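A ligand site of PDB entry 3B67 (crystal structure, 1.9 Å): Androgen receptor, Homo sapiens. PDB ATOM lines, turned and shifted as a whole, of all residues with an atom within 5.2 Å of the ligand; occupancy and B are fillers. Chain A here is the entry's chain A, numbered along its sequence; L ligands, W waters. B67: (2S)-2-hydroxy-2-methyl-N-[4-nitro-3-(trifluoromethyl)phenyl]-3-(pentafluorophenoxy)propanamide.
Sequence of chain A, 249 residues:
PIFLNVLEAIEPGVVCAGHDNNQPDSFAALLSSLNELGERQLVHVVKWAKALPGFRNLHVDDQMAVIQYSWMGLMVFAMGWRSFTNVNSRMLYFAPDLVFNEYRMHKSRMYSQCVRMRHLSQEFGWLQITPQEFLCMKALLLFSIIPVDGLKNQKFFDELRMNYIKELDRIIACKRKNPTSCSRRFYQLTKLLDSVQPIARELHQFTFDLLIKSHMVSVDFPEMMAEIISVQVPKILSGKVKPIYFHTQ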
ATOM      1  N   LEU A  31     -24.493 -26.653 -29.547  1.00  0.00           N
ATOM      2  CA  LEU A  31     -25.778 -26.243 -29.012  1.00  0.00           C
ATOM      3  C   LEU A  31     -26.688 -27.436 -28.741  1.00  0.00           C
ATOM      4  O   LEU A  31     -27.507 -27.395 -27.814  1.00  0.00           O
ATOM      5  CB  LEU A  31     -26.490 -25.264 -29.961  1.00  0.00           C
ATOM      6  CG  LEU A  31     -26.286 -23.777 -29.653  1.00  0.00           C
ATOM      7  CD1 LEU A  31     -26.824 -23.459 -28.250  1.00  0.00           C
ATOM      8  CD2 LEU A  31     -24.800 -23.430 -29.738  1.00  0.00           C
ATOM      9  N   LEU A  34     -25.591 -28.577 -25.551  1.00  0.00           N
ATOM     10  CA  LEU A  34     -25.982 -27.672 -24.481  1.00  0.00           C
ATOM     11  C   LEU A  34     -27.450 -27.871 -24.133  1.00  0.00           C
ATOM     12  O   LEU A  34     -27.808 -27.765 -22.967  1.00  0.00           O
ATOM     13  CB  LEU A  34     -25.748 -26.201 -24.871  1.00  0.00           C
ATOM     14  CG  LEU A  34     -24.354 -25.620 -24.614  1.00  0.00           C
ATOM     15  CD1 LEU A  34     -24.241 -24.253 -25.255  1.00  0.00           C
ATOM     16  CD2 LEU A  34     -24.090 -25.558 -23.113  1.00  0.00           C
ATOM     17  N   ASN A  35     -28.282 -28.137 -25.137  1.00  0.00           N
ATOM     18  CA  ASN A  35     -29.722 -28.349 -24.926  1.00  0.00           C
ATOM     19  C   ASN A  35     -29.932 -29.668 -24.192  1.00  0.00           C
ATOM     20  O   ASN A  35     -30.703 -29.731 -23.246  1.00  0.00           O
ATOM     21  CB  ASN A  35     -30.492 -28.386 -26.255  1.00  0.00           C
ATOM     22  CG  ASN A  35     -30.520 -27.042 -26.968  1.00  0.00           C
ATOM     23  OD1 ASN A  35     -30.419 -26.000 -26.334  1.00  0.00           O
ATOM     24  ND2 ASN A  35     -30.697 -27.076 -28.278  1.00  0.00           N
ATOM     25  N   LEU A  37     -27.808 -31.331 -22.336  1.00  0.00           N
ATOM     26  CA  LEU A  37     -27.297 -31.157 -20.986  1.00  0.00           C
ATOM     27  C   LEU A  37     -28.325 -30.395 -20.148  1.00  0.00           C
ATOM     28  O   LEU A  37     -28.659 -30.804 -19.026  1.00  0.00           O
ATOM     29  CB  LEU A  37     -25.964 -30.383 -21.019  1.00  0.00           C
ATOM     30  CG  LEU A  37     -25.390 -29.990 -19.658  1.00  0.00           C
ATOM     31  CD1 LEU A  37     -25.061 -31.256 -18.840  1.00  0.00           C
ATOM     32  CD2 LEU A  37     -24.155 -29.139 -19.849  1.00  0.00           C
ATOM     33  N   GLY A  38     -28.833 -29.293 -20.695  1.00  0.00           N
ATOM     34  CA  GLY A  38     -29.818 -28.504 -19.984  1.00  0.00           C
ATOM     35  C   GLY A  38     -30.984 -29.341 -19.515  1.00  0.00           C
ATOM     36  O   GLY A  38     -31.466 -29.195 -18.384  1.00  0.00           O
ATOM     37  N   GLN A  41     -29.954 -31.701 -16.751  1.00  0.00           N
ATOM     38  CA  GLN A  41     -29.822 -30.902 -15.541  1.00  0.00           C
ATOM     39  C   GLN A  41     -31.155 -30.526 -14.900  1.00  0.00           C
ATOM     40  O   GLN A  41     -31.311 -30.613 -13.672  1.00  0.00           O
ATOM     41  CB  GLN A  41     -28.976 -29.645 -15.840  1.00  0.00           C
ATOM     42  CG  GLN A  41     -27.473 -29.977 -15.935  1.00  0.00           C
ATOM     43  CD  GLN A  41     -26.607 -28.806 -16.391  1.00  0.00           C
ATOM     44  OE1 GLN A  41     -25.418 -28.744 -16.095  1.00  0.00           O
ATOM     45  NE2 GLN A  41     -27.203 -27.893 -17.143  1.00  0.00           N
ATOM     46  N   GLN A  68     -39.089 -23.287 -13.017  1.00  0.00           N
ATOM     47  CA  GLN A  68     -38.861 -22.986 -14.418  1.00  0.00           C
ATOM     48  C   GLN A  68     -38.351 -21.567 -14.654  1.00  0.00           C
ATOM     49  O   GLN A  68     -37.514 -21.340 -15.528  1.00  0.00           O
ATOM     50  CB  GLN A  68     -40.149 -23.243 -15.208  1.00  0.00           C
ATOM     51  CG  GLN A  68     -40.746 -24.603 -14.885  1.00  0.00           C
ATOM     52  CD  GLN A  68     -41.941 -24.964 -15.753  1.00  0.00           C
ATOM     53  OE1 GLN A  68     -42.838 -24.158 -15.962  1.00  0.00           O
ATOM     54  NE2 GLN A  68     -41.945 -26.193 -16.246  1.00  0.00           N
ATOM     55  N   TRP A  71     -34.694 -21.453 -13.187  1.00  0.00           N
ATOM     56  CA  TRP A  71     -33.833 -22.463 -13.777  1.00  0.00           C
ATOM     57  C   TRP A  71     -32.502 -21.928 -14.346  1.00  0.00           C
ATOM     58  O   TRP A  71     -31.430 -22.355 -13.931  1.00  0.00           O
ATOM     59  CB  TRP A  71     -34.642 -23.237 -14.831  1.00  0.00           C
ATOM     60  CG  TRP A  71     -33.920 -24.319 -15.582  1.00  0.00           C
ATOM     61  CD1 TRP A  71     -32.808 -25.010 -15.191  1.00  0.00           C
ATOM     62  CD2 TRP A  71     -34.272 -24.850 -16.872  1.00  0.00           C
ATOM     63  NE1 TRP A  71     -32.444 -25.925 -16.151  1.00  0.00           N
ATOM     64  CE2 TRP A  71     -33.328 -25.841 -17.201  1.00  0.00           C
ATOM     65  CE3 TRP A  71     -35.310 -24.567 -17.787  1.00  0.00           C
ATOM     66  CZ2 TRP A  71     -33.381 -26.563 -18.397  1.00  0.00           C
ATOM     67  CZ3 TRP A  71     -35.358 -25.282 -18.977  1.00  0.00           C
ATOM     68  CH2 TRP A  71     -34.401 -26.267 -19.271  1.00  0.00           C
ATOM     69  N   MET A  72     -32.576 -20.971 -15.273  1.00  0.00           N
ATOM     70  CA  MET A  72     -31.361 -20.421 -15.891  1.00  0.00           C
ATOM     71  C   MET A  72     -30.361 -19.822 -14.909  1.00  0.00           C
ATOM     72  O   MET A  72     -29.177 -20.134 -14.973  1.00  0.00           O
ATOM     73  CB  MET A  72     -31.727 -19.363 -16.942  1.00  0.00           C
ATOM     74  CG  MET A  72     -30.540 -18.908 -17.804  1.00  0.00           C
ATOM     75  SD  MET A  72     -29.950 -20.200 -18.944  1.00  0.00           S
ATOM     76  CE  MET A  72     -31.011 -19.861 -20.389  1.00  0.00           C
ATOM     77  N   MET A  75     -28.466 -22.463 -12.767  1.00  0.00           N
ATOM     78  CA  MET A  75     -27.451 -23.141 -13.565  1.00  0.00           C
ATOM     79  C   MET A  75     -26.241 -22.256 -13.787  1.00  0.00           C
ATOM     80  O   MET A  75     -25.105 -22.697 -13.636  1.00  0.00           O
ATOM     81  CB  MET A  75     -28.039 -23.537 -14.909  1.00  0.00           C
ATOM     82  CG  MET A  75     -29.336 -24.285 -14.795  1.00  0.00           C
ATOM     83  SD  MET A  75     -29.118 -26.050 -14.938  1.00  0.00           S
ATOM     84  CE  MET A  75     -29.422 -26.237 -16.745  1.00  0.00           C
ATOM     85  N   VAL A  76     -26.489 -21.020 -14.162  1.00  0.00           N
ATOM     86  CA  VAL A  76     -25.435 -20.067 -14.404  1.00  0.00           C
ATOM     87  C   VAL A  76     -24.533 -19.977 -13.173  1.00  0.00           C
ATOM     88  O   VAL A  76     -23.306 -20.024 -13.275  1.00  0.00           O
ATOM     89  CB  VAL A  76     -26.004 -18.662 -14.699  1.00  0.00           C
ATOM     90  CG1 VAL A  76     -24.902 -17.609 -14.650  1.00  0.00           C
ATOM     91  CG2 VAL A  76     -26.671 -18.651 -16.057  1.00  0.00           C
ATOM     92  N   MET A  79     -22.711 -23.410 -12.542  1.00  0.00           N
ATOM     93  CA  MET A  79     -21.696 -23.622 -13.570  1.00  0.00           C
ATOM     94  C   MET A  79     -20.495 -22.717 -13.319  1.00  0.00           C
ATOM     95  O   MET A  79     -19.356 -23.115 -13.563  1.00  0.00           O
ATOM     96  CB  MET A  79     -22.306 -23.349 -14.960  1.00  0.00           C
ATOM     97  CG  MET A  79     -21.438 -23.770 -16.147  1.00  0.00           C
ATOM     98  SD  MET A  79     -20.103 -22.626 -16.555  1.00  0.00           S
ATOM     99  CE  MET A  79     -20.957 -21.414 -17.510  1.00  0.00           C
ATOM    100  N   ARG A  82     -18.532 -24.237 -10.566  1.00  0.00           N
ATOM    101  CA  ARG A  82     -17.839 -25.416 -11.086  1.00  0.00           C
ATOM    102  C   ARG A  82     -16.596 -24.997 -11.870  1.00  0.00           C
ATOM    103  O   ARG A  82     -15.556 -25.647 -11.801  1.00  0.00           O
ATOM    104  CB  ARG A  82     -18.741 -26.228 -12.007  1.00  0.00           C
ATOM    105  CG  ARG A  82     -19.717 -27.150 -11.297  1.00  0.00           C
ATOM    106  CD  ARG A  82     -20.184 -28.275 -12.241  1.00  0.00           C
ATOM    107  NE  ARG A  82     -20.833 -27.767 -13.450  1.00  0.00           N
ATOM    108  CZ  ARG A  82     -22.073 -27.282 -13.479  1.00  0.00           C
ATOM    109  NH1 ARG A  82     -22.795 -27.245 -12.370  1.00  0.00           N
ATOM    110  NH2 ARG A  82     -22.600 -26.854 -14.622  1.00  0.00           N
ATOM    111  N   PHE A  94     -19.252 -26.435 -18.151  1.00  0.00           N
ATOM    112  CA  PHE A  94     -20.683 -26.743 -18.200  1.00  0.00           C
ATOM    113  C   PHE A  94     -20.906 -28.159 -17.686  1.00  0.00           C
ATOM    114  O   PHE A  94     -21.878 -28.446 -16.991  1.00  0.00           O
ATOM    115  CB  PHE A  94     -21.207 -26.644 -19.636  1.00  0.00           C
ATOM    116  CG  PHE A  94     -21.189 -25.259 -20.205  1.00  0.00           C
ATOM    117  CD1 PHE A  94     -20.071 -24.778 -20.885  1.00  0.00           C
ATOM    118  CD2 PHE A  94     -22.319 -24.450 -20.101  1.00  0.00           C
ATOM    119  CE1 PHE A  94     -20.088 -23.516 -21.459  1.00  0.00           C
ATOM    120  CE2 PHE A  94     -22.330 -23.182 -20.670  1.00  0.00           C
ATOM    121  CZ  PHE A  94     -21.215 -22.715 -21.349  1.00  0.00           C
ATOM    122  N   MET A 110     -22.216 -17.596 -28.364  1.00  0.00           N
ATOM    123  CA  MET A 110     -22.678 -17.147 -27.042  1.00  0.00           C
ATOM    124  C   MET A 110     -21.507 -16.499 -26.319  1.00  0.00           C
ATOM    125  O   MET A 110     -21.457 -16.486 -25.098  1.00  0.00           O
ATOM    126  CB  MET A 110     -23.149 -18.325 -26.201  1.00  0.00           C
ATOM    127  CG  MET A 110     -24.126 -19.251 -26.879  1.00  0.00           C
ATOM    128  SD  MET A 110     -24.451 -20.703 -25.844  1.00  0.00           S
ATOM    129  CE  MET A 110     -25.448 -19.997 -24.591  1.00  0.00           C
ATOM    130  N   MET A 117     -20.124 -14.945 -17.691  1.00  0.00           N
ATOM    131  CA  MET A 117     -20.133 -16.081 -16.783  1.00  0.00           C
ATOM    132  C   MET A 117     -18.722 -16.411 -16.285  1.00  0.00           C
ATOM    133  O   MET A 117     -18.554 -16.832 -15.128  1.00  0.00           O
ATOM    134  CB  MET A 117     -20.764 -17.301 -17.459  1.00  0.00           C
ATOM    135  CG  MET A 117     -22.240 -17.118 -17.724  1.00  0.00           C
ATOM    136  SD  MET A 117     -23.094 -18.640 -18.196  1.00  0.00           S
ATOM    137  CE  MET A 117     -22.629 -18.749 -19.914  1.00  0.00           C
ATOM    138  N   LEU A 203     -28.964 -15.075 -21.719  1.00  0.00           N
ATOM    139  CA  LEU A 203     -28.999 -16.441 -22.186  1.00  0.00           C
ATOM    140  C   LEU A 203     -30.414 -16.769 -22.662  1.00  0.00           C
ATOM    141  O   LEU A 203     -30.588 -17.439 -23.673  1.00  0.00           O
ATOM    142  CB  LEU A 203     -28.549 -17.390 -21.072  1.00  0.00           C
ATOM    143  CG  LEU A 203     -27.032 -17.377 -20.782  1.00  0.00           C
ATOM    144  CD1 LEU A 203     -26.763 -17.977 -19.427  1.00  0.00           C
ATOM    145  CD2 LEU A 203     -26.273 -18.132 -21.876  1.00  0.00           C
ATOM    146  N   HIS A 204     -31.398 -16.282 -21.911  1.00  0.00           N
ATOM    147  CA  HIS A 204     -32.817 -16.484 -22.221  1.00  0.00           C
ATOM    148  C   HIS A 204     -33.132 -15.972 -23.630  1.00  0.00           C
ATOM    149  O   HIS A 204     -33.737 -16.668 -24.447  1.00  0.00           O
ATOM    150  CB  HIS A 204     -33.694 -15.731 -21.228  1.00  0.00           C
ATOM    151  CG  HIS A 204     -33.982 -16.491 -19.979  1.00  0.00           C
ATOM    152  ND1 HIS A 204     -34.093 -15.884 -18.746  1.00  0.00           N
ATOM    153  CD2 HIS A 204     -34.236 -17.808 -19.767  1.00  0.00           C
ATOM    154  CE1 HIS A 204     -34.400 -16.789 -17.836  1.00  0.00           C
ATOM    155  NE2 HIS A 204     -34.496 -17.960 -18.433  1.00  0.00           N
ATOM    156  N   PHE A 206     -31.022 -15.300 -25.999  1.00  0.00           N
ATOM    157  CA  PHE A 206     -30.283 -16.108 -26.958  1.00  0.00           C
ATOM    158  C   PHE A 206     -31.025 -17.403 -27.220  1.00  0.00           C
ATOM    159  O   PHE A 206     -31.230 -17.792 -28.365  1.00  0.00           O
ATOM    160  CB  PHE A 206     -28.875 -16.405 -26.421  1.00  0.00           C
ATOM    161  CG  PHE A 206     -28.159 -17.493 -27.160  1.00  0.00           C
ATOM    162  CD1 PHE A 206     -28.278 -18.815 -26.765  1.00  0.00           C
ATOM    163  CD2 PHE A 206     -27.368 -17.190 -28.276  1.00  0.00           C
ATOM    164  CE1 PHE A 206     -27.628 -19.835 -27.463  1.00  0.00           C
ATOM    165  CE2 PHE A 206     -26.717 -18.190 -28.982  1.00  0.00           C
ATOM    166  CZ  PHE A 206     -26.842 -19.517 -28.575  1.00  0.00           C
ATOM    167  N   THR A 207     -31.434 -18.060 -26.155  1.00  0.00           N
ATOM    168  CA  THR A 207     -32.146 -19.332 -26.274  1.00  0.00           C
ATOM    169  C   THR A 207     -33.470 -19.180 -27.014  1.00  0.00           C
ATOM    170  O   THR A 207     -33.837 -20.016 -27.845  1.00  0.00           O
ATOM    171  CB  THR A 207     -32.429 -19.926 -24.896  1.00  0.00           C
ATOM    172  OG1 THR A 207     -31.192 -20.223 -24.231  1.00  0.00           O
ATOM    173  CG2 THR A 207     -33.242 -21.186 -25.042  1.00  0.00           C
ATOM    174  N   MET A 225     -37.791 -28.782 -22.635  1.00  0.00           N
ATOM    175  CA  MET A 225     -37.115 -27.511 -22.806  1.00  0.00           C
ATOM    176  C   MET A 225     -37.903 -26.594 -23.736  1.00  0.00           C
ATOM    177  O   MET A 225     -38.224 -25.461 -23.378  1.00  0.00           O
ATOM    178  CB  MET A 225     -35.710 -27.738 -23.361  1.00  0.00           C
ATOM    179  CG  MET A 225     -34.883 -26.496 -23.481  1.00  0.00           C
ATOM    180  SD  MET A 225     -33.177 -26.876 -23.916  1.00  0.00           S
ATOM    181  CE  MET A 225     -32.569 -27.470 -22.315  1.00  0.00           C
ATOM    182  N   ILE A 228     -40.849 -25.005 -22.159  1.00  0.00           N
ATOM    183  CA  ILE A 228     -40.499 -23.956 -21.213  1.00  0.00           C
ATOM    184  C   ILE A 228     -40.084 -22.672 -21.923  1.00  0.00           C
ATOM    185  O   ILE A 228     -40.477 -21.572 -21.513  1.00  0.00           O
ATOM    186  CB  ILE A 228     -39.361 -24.412 -20.268  1.00  0.00           C
ATOM    187  CG1 ILE A 228     -39.927 -25.414 -19.249  1.00  0.00           C
ATOM    188  CG2 ILE A 228     -38.720 -23.202 -19.592  1.00  0.00           C
ATOM    189  CD1 ILE A 228     -38.888 -26.068 -18.358  1.00  0.00           C
ATOM    190  N   ILE A 229     -39.299 -22.815 -22.990  1.00  0.00           N
ATOM    191  CA  ILE A 229     -38.832 -21.669 -23.754  1.00  0.00           C
ATOM    192  C   ILE A 229     -39.984 -20.942 -24.438  1.00  0.00           C
ATOM    193  O   ILE A 229     -39.985 -19.715 -24.518  1.00  0.00           O
ATOM    194  CB  ILE A 229     -37.841 -22.105 -24.862  1.00  0.00           C
ATOM    195  CG1 ILE A 229     -36.623 -22.784 -24.243  1.00  0.00           C
ATOM    196  CG2 ILE A 229     -37.404 -20.890 -25.677  1.00  0.00           C
ATOM    197  CD1 ILE A 229     -35.625 -23.289 -25.259  1.00  0.00           C
ATOM    198  N   VAL A 233     -40.257 -18.704 -20.807  1.00  0.00           N
ATOM    199  CA  VAL A 233     -39.259 -17.669 -21.107  1.00  0.00           C
ATOM    200  C   VAL A 233     -39.836 -16.397 -21.730  1.00  0.00           C
ATOM    201  O   VAL A 233     -39.318 -15.307 -21.482  1.00  0.00           O
ATOM    202  CB  VAL A 233     -38.129 -18.239 -21.995  1.00  0.00           C
ATOM    203  CG1 VAL A 233     -37.123 -17.135 -22.328  1.00  0.00           C
ATOM    204  CG2 VAL A 233     -37.440 -19.399 -21.267  1.00  0.00           C
HETATM  205  F1  B67 L   1     -25.849 -21.239 -19.145  1.00  0.00           F
HETATM  206  C7  B67 L   1     -25.644 -22.259 -18.309  1.00  0.00           C
HETATM  207  F2  B67 L   1     -26.398 -22.051 -17.240  1.00  0.00           F
HETATM  208  F3  B67 L   1     -24.359 -22.193 -17.965  1.00  0.00           F
HETATM  209  C4  B67 L   1     -25.997 -23.603 -18.965  1.00  0.00           C
HETATM  210  C5  B67 L   1     -26.767 -23.594 -20.129  1.00  0.00           C
HETATM  211  C3  B67 L   1     -25.519 -24.842 -18.520  1.00  0.00           C
HETATM  212  N8  B67 L   1     -24.967 -25.026 -17.322  1.00  0.00           N
HETATM  213  O2  B67 L   1     -24.411 -26.296 -17.024  1.00  0.00           O
HETATM  214  O1  B67 L   1     -24.826 -23.995 -16.351  1.00  0.00           O
HETATM  215  C2  B67 L   1     -25.807 -25.993 -19.244  1.00  0.00           C
HETATM  216  C1  B67 L   1     -26.569 -25.964 -20.403  1.00  0.00           C
HETATM  217  C6  B67 L   1     -27.069 -24.750 -20.853  1.00  0.00           C
HETATM  218  N9  B67 L   1     -27.877 -24.742 -21.908  1.00  0.00           N
HETATM  219  C10 B67 L   1     -28.470 -23.655 -22.410  1.00  0.00           C
HETATM  220  O10 B67 L   1     -28.346 -22.520 -21.960  1.00  0.00           O
HETATM  221  C11 B67 L   1     -29.376 -23.917 -23.618  1.00  0.00           C
HETATM  222  O11 B67 L   1     -29.280 -25.299 -23.995  1.00  0.00           O
HETATM  223  C12 B67 L   1     -28.961 -23.021 -24.785  1.00  0.00           C
HETATM  224  C13 B67 L   1     -30.810 -23.598 -23.214  1.00  0.00           C
HETATM  225  O14 B67 L   1     -31.335 -24.494 -22.229  1.00  0.00           O
HETATM  226  C16 B67 L   1     -31.916 -23.832 -21.183  1.00  0.00           C
HETATM  227  C17 B67 L   1     -31.290 -23.784 -19.945  1.00  0.00           C
HETATM  228  F17 B67 L   1     -30.087 -24.385 -19.817  1.00  0.00           F
HETATM  229  C18 B67 L   1     -31.904 -23.134 -18.870  1.00  0.00           C
HETATM  230  F18 B67 L   1     -31.311 -23.145 -17.658  1.00  0.00           F
HETATM  231  C19 B67 L   1     -33.142 -22.514 -19.058  1.00  0.00           C
HETATM  232  F19 B67 L   1     -33.709 -21.827 -18.036  1.00  0.00           F
HETATM  233  C20 B67 L   1     -33.773 -22.569 -20.302  1.00  0.00           C
HETATM  234  F20 B67 L   1     -34.947 -21.919 -20.495  1.00  0.00           F
HETATM  235  C21 B67 L   1     -33.163 -23.231 -21.358  1.00  0.00           C
HETATM  236  F21 B67 L   1     -33.765 -23.377 -22.561  1.00  0.00           F
HETATM  237  O   HOH W   1     -25.276 -25.653 -13.762  1.00  0.00           O
HETATM  238  O   HOH W   2     -35.433 -19.787 -16.227  1.00  0.00           O
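The backbone NH (N) of Asn 35 lies within hydrogen-bond range of an oxygen (O11) of the ligand, at 3.2 Å. An oxygen (O11) of the ligand is in hydrogen-bond range of the side-chain amide oxygen (OD1) of Asn 35 (2.7 Å). The side-chain amide oxygen of Gln 41 lies close to an oxygen (O2) of the ligand. The backbone carbonyl oxygen (O) of Leu 34 is in hydrogen-bond range of an oxygen (O11) of the ligand, at 3.1 Å. O2 of the ligand lies within hydrogen-bond range of NH2 of Arg 82 (3.1 Å).
The side-chain sulfur of Met 225 lies close to the side-chain amide oxygen of Asn 35 (3.8 Å). The side-chain amide nitrogen of Asn 35 sits close to the backbone carbonyl oxygen of Leu 31, 3.2 Å away. NE2 of Gln 41 sits close to SD of Met 75. The side-chain sulfur (SD) of Met 75 sits close to the indole nitrogen (NE1) of Trp 71 (3.5 Å). The guanidinium group (NH2) of Arg 82 sits at hydrogen-bond distance from the backbone carbonyl oxygen (O) of Phe 94, at 2.9 Å. OG1 of Thr 207 is in hydrogen-bond range of O of Leu 203. N of Val 233 lies within hydrogen-bond range of O of Ile 228 (3.0 Å).
A fluorine (F18) of the ligand sits close to the indole nitrogen of Trp 71 (3.4 Å). N of Met 72 lies close to F19 of the ligand. O1 of the ligand sits close to O of Met 75, at 3.0 Å. N of Val 76 sits close to F2 of the ligand. The backbone carbonyl oxygen (O) of Phe 94 sits close to an oxygen (O2) of the ligand (3.3 Å). SD of Met 117 lies close to F3 of the ligand, 3.8 Å away. SD of Met 225 lies close to O14 of the ligand (3.5 Å). Residues that only touch the ligand: Leu 37, Met 79, Leu 203, His 204, Thr 207, Ile 229 and Val 233. Hydrophobic or aromatic side chains within 4 Å of the ligand: Leu 34, Leu 37, Trp 71, Met 72, Met 75, Val 76, Met 79, Phe 94, Met 117, Leu 203, Met 225, Ile 229 and Val 233. Within 4 Å of the ligand: Leu 34, Asn 35, Leu 37, Gln 41, Trp 71, Met 72, Met 75, Val 76, Met 79, Arg 82, Phe 94, Met 117, Leu 203, His 204, Thr 207, Met 225, Ile 229 and Val 233. The nearest printed residue that does not touch the ligand is Gly 38 (4.04 Å).
Water W1 lies within hydrogen-bond range of the backbone carbonyl oxygen (O) of Met 75, the guanidinium group (NH2) of Arg 82 and an oxygen (O1) of the ligand. Water W2 lies within hydrogen-bond range of the backbone carbonyl oxygen (O) of Gln 68 (2.7 Å), a ring nitrogen (NE2) of His 204 (3.0 Å) and the backbone NH (N) of Met 72 (3.2 Å).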
